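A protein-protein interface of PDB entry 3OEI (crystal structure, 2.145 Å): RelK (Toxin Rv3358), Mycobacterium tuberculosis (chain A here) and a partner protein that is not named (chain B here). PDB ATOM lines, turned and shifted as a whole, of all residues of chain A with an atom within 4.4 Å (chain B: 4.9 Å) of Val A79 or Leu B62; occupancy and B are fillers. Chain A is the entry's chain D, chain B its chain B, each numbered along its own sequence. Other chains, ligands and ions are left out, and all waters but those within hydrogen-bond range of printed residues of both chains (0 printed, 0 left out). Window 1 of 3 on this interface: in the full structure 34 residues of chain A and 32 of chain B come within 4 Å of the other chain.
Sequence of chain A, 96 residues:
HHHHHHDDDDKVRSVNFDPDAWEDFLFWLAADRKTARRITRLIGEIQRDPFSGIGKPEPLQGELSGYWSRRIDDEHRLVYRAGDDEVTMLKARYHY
The side-chain amino group of Lys A91 sits close to the guanidinium group of Arg B61 (2.9 Å).
Among the printed residues, pairs that only touch across the chains: Leu A64 with Leu B62, Leu A64 with Met B63, Leu A64 with Val B66, Arg A77 with Leu B52, Val A79 with Leu B62, Leu A90 with Ala B65 and Leu A90 with Val B66.
The backbone carbonyl oxygen (O) of Leu B52 lies within hydrogen-bond range of the side-chain amide nitrogen (ND2) of Asn B58 (2.9 Å). The backbone carbonyl oxygen of Val A79 is in hydrogen-bond range of the backbone NH of Leu A90, at 2.8 Å. The backbone NH of Val A79 is in hydrogen-bond range of the backbone carbonyl oxygen of Lys A91 (2.7 Å).
Of the printed residues of chain B, Val A79 touches Leu B62 (3.8 Å). Leu B62 touches just these residues of chain A: Leu A64 (3.96 Å) and Val A79 (3.8 Å). Of the printed residues of chain A, Ala B65 touches Leu A90 (3.6 Å). Printed residues of chain B within 4 Å of Arg A77: Leu B52. Printed residues of chain B within 4 Å of Leu A90: Ala B65 (3.6 Å) and Val B66 (3.6 Å). Of the printed residues of chain A, Met B63 touches Leu A64 (3.5 Å). The nearest residue of chain B that does not touch Val A79 is Leu B52 (4.3 Å).
Hydrophobic or aromatic side chains of chain A that line the printed part of chain B: Leu A64, Val A79 and Leu A90. Among the printed residues, 8 pairs touch across the chains.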
ATOM      1  N   LEU A  64      -8.270  -7.385  -6.720  1.00  0.00           N
ATOM      2  CA  LEU A  64      -8.529  -7.098  -8.118  1.00  0.00           C
ATOM      3  C   LEU A  64      -9.917  -7.592  -8.557  1.00  0.00           C
ATOM      4  O   LEU A  64     -10.260  -7.576  -9.735  1.00  0.00           O
ATOM      5  CB  LEU A  64      -7.425  -7.691  -8.981  1.00  0.00           C
ATOM      6  CG  LEU A  64      -6.127  -6.904  -8.889  1.00  0.00           C
ATOM      7  CD1 LEU A  64      -4.964  -7.697  -9.499  1.00  0.00           C
ATOM      8  CD2 LEU A  64      -6.317  -5.532  -9.595  1.00  0.00           C
ATOM      9  N   TRP A  68     -10.893  -8.268 -15.179  1.00  0.00           N
ATOM     10  CA  TRP A  68     -10.611  -9.452 -15.956  1.00  0.00           C
ATOM     11  C   TRP A  68      -9.278  -9.294 -16.662  1.00  0.00           C
ATOM     12  O   TRP A  68      -8.828  -8.181 -16.915  1.00  0.00           O
ATOM     13  CB  TRP A  68     -11.727  -9.691 -16.992  1.00  0.00           C
ATOM     14  CG  TRP A  68     -12.977 -10.224 -16.395  1.00  0.00           C
ATOM     15  CD1 TRP A  68     -13.892  -9.528 -15.656  1.00  0.00           C
ATOM     16  CD2 TRP A  68     -13.463 -11.574 -16.476  1.00  0.00           C
ATOM     17  NE1 TRP A  68     -14.909 -10.359 -15.270  1.00  0.00           N
ATOM     18  CE2 TRP A  68     -14.675 -11.618 -15.758  1.00  0.00           C
ATOM     19  CE3 TRP A  68     -12.995 -12.743 -17.086  1.00  0.00           C
ATOM     20  CZ2 TRP A  68     -15.425 -12.788 -15.635  1.00  0.00           C
ATOM     21  CZ3 TRP A  68     -13.740 -13.901 -16.969  1.00  0.00           C
ATOM     22  CH2 TRP A  68     -14.941 -13.917 -16.246  1.00  0.00           C
ATOM     23  N   ARG A  77      -0.553  -8.853 -20.621  1.00  0.00           N
ATOM     24  CA  ARG A  77      -1.973  -9.007 -20.368  1.00  0.00           C
ATOM     25  C   ARG A  77      -2.722  -7.693 -20.576  1.00  0.00           C
ATOM     26  O   ARG A  77      -2.236  -6.630 -20.244  1.00  0.00           O
ATOM     27  CB  ARG A  77      -2.187  -9.495 -18.939  1.00  0.00           C
ATOM     28  CG  ARG A  77      -1.393 -10.740 -18.596  1.00  0.00           C
ATOM     29  CD  ARG A  77      -1.979 -11.966 -19.264  1.00  0.00           C
ATOM     30  NE  ARG A  77      -1.480 -13.205 -18.668  1.00  0.00           N
ATOM     31  CZ  ARG A  77      -0.423 -13.874 -19.123  1.00  0.00           C
ATOM     32  NH1 ARG A  77       0.241 -13.430 -20.187  1.00  0.00           N
ATOM     33  NH2 ARG A  77      -0.031 -14.998 -18.531  1.00  0.00           N
ATOM     34  N   LEU A  78      -3.913  -7.794 -21.142  1.00  0.00           N
ATOM     35  CA  LEU A  78      -4.828  -6.687 -21.253  1.00  0.00           C
ATOM     36  C   LEU A  78      -5.753  -6.824 -20.062  1.00  0.00           C
ATOM     37  O   LEU A  78      -6.455  -7.825 -19.937  1.00  0.00           O
ATOM     38  CB  LEU A  78      -5.617  -6.835 -22.549  1.00  0.00           C
ATOM     39  CG  LEU A  78      -6.657  -5.787 -22.944  1.00  0.00           C
ATOM     40  CD1 LEU A  78      -6.034  -4.391 -23.116  1.00  0.00           C
ATOM     41  CD2 LEU A  78      -7.331  -6.245 -24.229  1.00  0.00           C
ATOM     42  N   VAL A  79      -5.740  -5.863 -19.147  1.00  0.00           N
ATOM     43  CA  VAL A  79      -6.661  -6.010 -18.042  1.00  0.00           C
ATOM     44  C   VAL A  79      -7.744  -4.956 -18.080  1.00  0.00           C
ATOM     45  O   VAL A  79      -7.507  -3.795 -18.407  1.00  0.00           O
ATOM     46  CB  VAL A  79      -5.981  -6.244 -16.648  1.00  0.00           C
ATOM     47  CG1 VAL A  79      -4.471  -6.377 -16.772  1.00  0.00           C
ATOM     48  CG2 VAL A  79      -6.409  -5.226 -15.649  1.00  0.00           C
ATOM     49  N   TYR A  80      -8.960  -5.400 -17.820  1.00  0.00           N
ATOM     50  CA  TYR A  80     -10.111  -4.577 -18.111  1.00  0.00           C
ATOM     51  C   TYR A  80     -11.257  -4.847 -17.161  1.00  0.00           C
ATOM     52  O   TYR A  80     -11.225  -5.789 -16.364  1.00  0.00           O
ATOM     53  CB  TYR A  80     -10.570  -4.808 -19.559  1.00  0.00           C
ATOM     54  CG  TYR A  80     -10.995  -6.223 -19.848  1.00  0.00           C
ATOM     55  CD1 TYR A  80     -10.052  -7.218 -20.113  1.00  0.00           C
ATOM     56  CD2 TYR A  80     -12.339  -6.567 -19.895  1.00  0.00           C
ATOM     57  CE1 TYR A  80     -10.444  -8.528 -20.394  1.00  0.00           C
ATOM     58  CE2 TYR A  80     -12.743  -7.869 -20.162  1.00  0.00           C
ATOM     59  CZ  TYR A  80     -11.792  -8.839 -20.416  1.00  0.00           C
ATOM     60  OH  TYR A  80     -12.193 -10.113 -20.690  1.00  0.00           O
ATOM     61  N   THR A  88     -13.763  -0.843 -19.978  1.00  0.00           N
ATOM     62  CA  THR A  88     -12.625   0.020 -19.661  1.00  0.00           C
ATOM     63  C   THR A  88     -11.329  -0.788 -19.629  1.00  0.00           C
ATOM     64  O   THR A  88     -11.239  -1.808 -18.963  1.00  0.00           O
ATOM     65  CB  THR A  88     -12.821   0.725 -18.300  1.00  0.00           C
ATOM     66  OG1 THR A  88     -14.011   1.511 -18.342  1.00  0.00           O
ATOM     67  CG2 THR A  88     -11.628   1.621 -17.952  1.00  0.00           C
ATOM     68  N   MET A  89     -10.328  -0.333 -20.364  1.00  0.00           N
ATOM     69  CA  MET A  89      -9.020  -0.950 -20.324  1.00  0.00           C
ATOM     70  C   MET A  89      -8.140  -0.225 -19.309  1.00  0.00           C
ATOM     71  O   MET A  89      -8.029   1.015 -19.341  1.00  0.00           O
ATOM     72  CB  MET A  89      -8.382  -0.884 -21.707  1.00  0.00           C
ATOM     73  CG  MET A  89      -9.334  -1.261 -22.831  1.00  0.00           C
ATOM     74  SD  MET A  89      -9.738  -3.014 -22.768  1.00  0.00           S
ATOM     75  CE  MET A  89     -11.488  -2.966 -23.162  1.00  0.00           C
ATOM     76  N   LEU A  90      -7.537  -0.996 -18.402  1.00  0.00           N
ATOM     77  CA  LEU A  90      -6.613  -0.458 -17.393  1.00  0.00           C
ATOM     78  C   LEU A  90      -5.144  -0.641 -17.754  1.00  0.00           C
ATOM     79  O   LEU A  90      -4.336   0.242 -17.495  1.00  0.00           O
ATOM     80  CB  LEU A  90      -6.894  -1.060 -16.021  1.00  0.00           C
ATOM     81  CG  LEU A  90      -8.105  -0.452 -15.313  1.00  0.00           C
ATOM     82  CD1 LEU A  90      -9.406  -0.977 -15.930  1.00  0.00           C
ATOM     83  CD2 LEU A  90      -8.041  -0.756 -13.825  1.00  0.00           C
ATOM     84  N   LYS A  91      -4.798  -1.773 -18.366  1.00  0.00           N
ATOM     85  CA  LYS A  91      -3.423  -2.019 -18.803  1.00  0.00           C
ATOM     86  C   LYS A  91      -3.382  -2.937 -20.016  1.00  0.00           C
ATOM     87  O   LYS A  91      -4.260  -3.800 -20.198  1.00  0.00           O
ATOM     88  CB  LYS A  91      -2.588  -2.641 -17.684  1.00  0.00           C
ATOM     89  CG  LYS A  91      -2.303  -1.729 -16.488  1.00  0.00           C
ATOM     90  CD  LYS A  91      -1.369  -0.576 -16.858  1.00  0.00           C
ATOM     91  CE  LYS A  91      -0.062  -1.118 -17.414  1.00  0.00           C
ATOM     92  NZ  LYS A  91       0.789  -0.036 -17.940  1.00  0.00           N
ATOM     93  N   LEU B  52      -0.057 -11.288 -12.148  1.00  0.00           N
ATOM     94  CA  LEU B  52      -0.058  -9.822 -12.282  1.00  0.00           C
ATOM     95  C   LEU B  52       0.620  -9.049 -11.129  1.00  0.00           C
ATOM     96  O   LEU B  52       1.202  -7.994 -11.349  1.00  0.00           O
ATOM     97  CB  LEU B  52      -1.477  -9.285 -12.495  1.00  0.00           C
ATOM     98  CG  LEU B  52      -2.115  -9.699 -13.826  1.00  0.00           C
ATOM     99  CD1 LEU B  52      -3.637  -9.460 -13.786  1.00  0.00           C
ATOM    100  CD2 LEU B  52      -1.466  -8.983 -15.020  1.00  0.00           C
ATOM    101  N   LEU B  53       0.528  -9.580  -9.912  1.00  0.00           N
ATOM    102  CA  LEU B  53       1.063  -8.924  -8.724  1.00  0.00           C
ATOM    103  C   LEU B  53       2.504  -9.291  -8.381  1.00  0.00           C
ATOM    104  O   LEU B  53       3.127  -8.617  -7.567  1.00  0.00           O
ATOM    105  CB  LEU B  53       0.188  -9.235  -7.516  1.00  0.00           C
ATOM    106  CG  LEU B  53      -1.242  -8.793  -7.763  1.00  0.00           C
ATOM    107  CD1 LEU B  53      -2.104  -9.096  -6.566  1.00  0.00           C
ATOM    108  CD2 LEU B  53      -1.228  -7.295  -8.085  1.00  0.00           C
ATOM    109  N   ASN B  58       4.971  -4.147 -11.906  1.00  0.00           N
ATOM    110  CA  ASN B  58       3.671  -4.363 -12.536  1.00  0.00           C
ATOM    111  C   ASN B  58       2.563  -4.104 -11.563  1.00  0.00           C
ATOM    112  O   ASN B  58       1.560  -3.498 -11.904  1.00  0.00           O
ATOM    113  CB  ASN B  58       3.517  -5.777 -13.113  1.00  0.00           C
ATOM    114  CG  ASN B  58       2.459  -5.830 -14.179  1.00  0.00           C
ATOM    115  OD1 ASN B  58       2.639  -5.267 -15.265  1.00  0.00           O
ATOM    116  ND2 ASN B  58       1.326  -6.478 -13.875  1.00  0.00           N
ATOM    117  N   ALA B  59       2.763  -4.569 -10.338  1.00  0.00           N
ATOM    118  CA  ALA B  59       1.756  -4.443  -9.299  1.00  0.00           C
ATOM    119  C   ALA B  59       1.502  -2.969  -9.082  1.00  0.00           C
ATOM    120  O   ALA B  59       0.357  -2.523  -8.955  1.00  0.00           O
ATOM    121  CB  ALA B  59       2.255  -5.101  -7.999  1.00  0.00           C
ATOM    122  N   ARG B  60       2.591  -2.209  -9.038  1.00  0.00           N
ATOM    123  CA  ARG B  60       2.494  -0.770  -8.843  1.00  0.00           C
ATOM    124  C   ARG B  60       1.708  -0.091  -9.964  1.00  0.00           C
ATOM    125  O   ARG B  60       0.764   0.656  -9.713  1.00  0.00           O
ATOM    126  CB  ARG B  60       3.887  -0.145  -8.729  1.00  0.00           C
ATOM    127  CG  ARG B  60       3.855   1.384  -8.772  1.00  0.00           C
ATOM    128  CD  ARG B  60       5.187   1.977  -8.370  1.00  0.00           C
ATOM    129  NE  ARG B  60       5.611   1.485  -7.057  1.00  0.00           N
ATOM    130  CZ  ARG B  60       5.159   1.953  -5.894  1.00  0.00           C
ATOM    131  NH1 ARG B  60       4.254   2.925  -5.865  1.00  0.00           N
ATOM    132  NH2 ARG B  60       5.612   1.450  -4.756  1.00  0.00           N
ATOM    133  N   ARG B  61       2.096  -0.352 -11.207  1.00  0.00           N
ATOM    134  CA  ARG B  61       1.431   0.289 -12.341  1.00  0.00           C
ATOM    135  C   ARG B  61      -0.056  -0.083 -12.405  1.00  0.00           C
ATOM    136  O   ARG B  61      -0.905   0.730 -12.782  1.00  0.00           O
ATOM    137  CB  ARG B  61       2.129  -0.090 -13.649  1.00  0.00           C
ATOM    138  CG  ARG B  61       3.441   0.633 -13.909  1.00  0.00           C
ATOM    139  CD  ARG B  61       3.162   2.047 -14.381  1.00  0.00           C
ATOM    140  NE  ARG B  61       4.142   2.517 -15.360  1.00  0.00           N
ATOM    141  CZ  ARG B  61       3.982   2.442 -16.680  1.00  0.00           C
ATOM    142  NH1 ARG B  61       2.883   1.902 -17.196  1.00  0.00           N
ATOM    143  NH2 ARG B  61       4.925   2.902 -17.492  1.00  0.00           N
ATOM    144  N   LEU B  62      -0.370  -1.306 -12.014  1.00  0.00           N
ATOM    145  CA  LEU B  62      -1.737  -1.814 -12.151  1.00  0.00           C
ATOM    146  C   LEU B  62      -2.669  -1.214 -11.116  1.00  0.00           C
ATOM    147  O   LEU B  62      -3.789  -0.809 -11.435  1.00  0.00           O
ATOM    148  CB  LEU B  62      -1.760  -3.345 -12.027  1.00  0.00           C
ATOM    149  CG  LEU B  62      -3.132  -4.032 -12.018  1.00  0.00           C
ATOM    150  CD1 LEU B  62      -4.052  -3.552 -13.156  1.00  0.00           C
ATOM    151  CD2 LEU B  62      -2.916  -5.528 -12.105  1.00  0.00           C
ATOM    152  N   MET B  63      -2.216  -1.178  -9.866  1.00  0.00           N
ATOM    153  CA  MET B  63      -3.037  -0.618  -8.796  1.00  0.00           C
ATOM    154  C   MET B  63      -3.202   0.911  -8.979  1.00  0.00           C
ATOM    155  O   MET B  63      -4.268   1.466  -8.715  1.00  0.00           O
ATOM    156  CB  MET B  63      -2.470  -0.995  -7.419  1.00  0.00           C
ATOM    157  CG  MET B  63      -2.397  -2.507  -7.187  1.00  0.00           C
ATOM    158  SD  MET B  63      -3.907  -3.342  -7.742  1.00  0.00           S
ATOM    159  CE  MET B  63      -3.403  -5.061  -7.752  1.00  0.00           C
ATOM    160  N   GLU B  64      -2.171   1.577  -9.481  1.00  0.00           N
ATOM    161  CA  GLU B  64      -2.339   2.980  -9.856  1.00  0.00           C
ATOM    162  C   GLU B  64      -3.477   3.131 -10.874  1.00  0.00           C
ATOM    163  O   GLU B  64      -4.372   3.966 -10.697  1.00  0.00           O
ATOM    164  CB  GLU B  64      -1.026   3.590 -10.363  1.00  0.00           C
ATOM    165  CG  GLU B  64       0.023   3.777  -9.248  1.00  0.00           C
ATOM    166  CD  GLU B  64       1.303   4.441  -9.743  1.00  0.00           C
ATOM    167  OE1 GLU B  64       1.270   5.055 -10.832  1.00  0.00           O
ATOM    168  OE2 GLU B  64       2.344   4.355  -9.042  1.00  0.00           O
ATOM    169  N   ALA B  65      -3.471   2.309 -11.923  1.00  0.00           N
ATOM    170  CA  ALA B  65      -4.590   2.322 -12.867  1.00  0.00           C
ATOM    171  C   ALA B  65      -5.911   1.973 -12.187  1.00  0.00           C
ATOM    172  O   ALA B  65      -6.961   2.545 -12.507  1.00  0.00           O
ATOM    173  CB  ALA B  65      -4.322   1.382 -14.067  1.00  0.00           C
ATOM    174  N   VAL B  66      -5.877   1.011 -11.267  1.00  0.00           N
ATOM    175  CA  VAL B  66      -7.109   0.599 -10.587  1.00  0.00           C
ATOM    176  C   VAL B  66      -7.657   1.724  -9.702  1.00  0.00           C
ATOM    177  O   VAL B  66      -8.876   1.939  -9.627  1.00  0.00           O
ATOM    178  CB  VAL B  66      -6.926  -0.652  -9.722  1.00  0.00           C
ATOM    179  CG1 VAL B  66      -8.192  -0.908  -8.922  1.00  0.00           C
ATOM    180  CG2 VAL B  66      -6.565  -1.863 -10.584  1.00  0.00           C
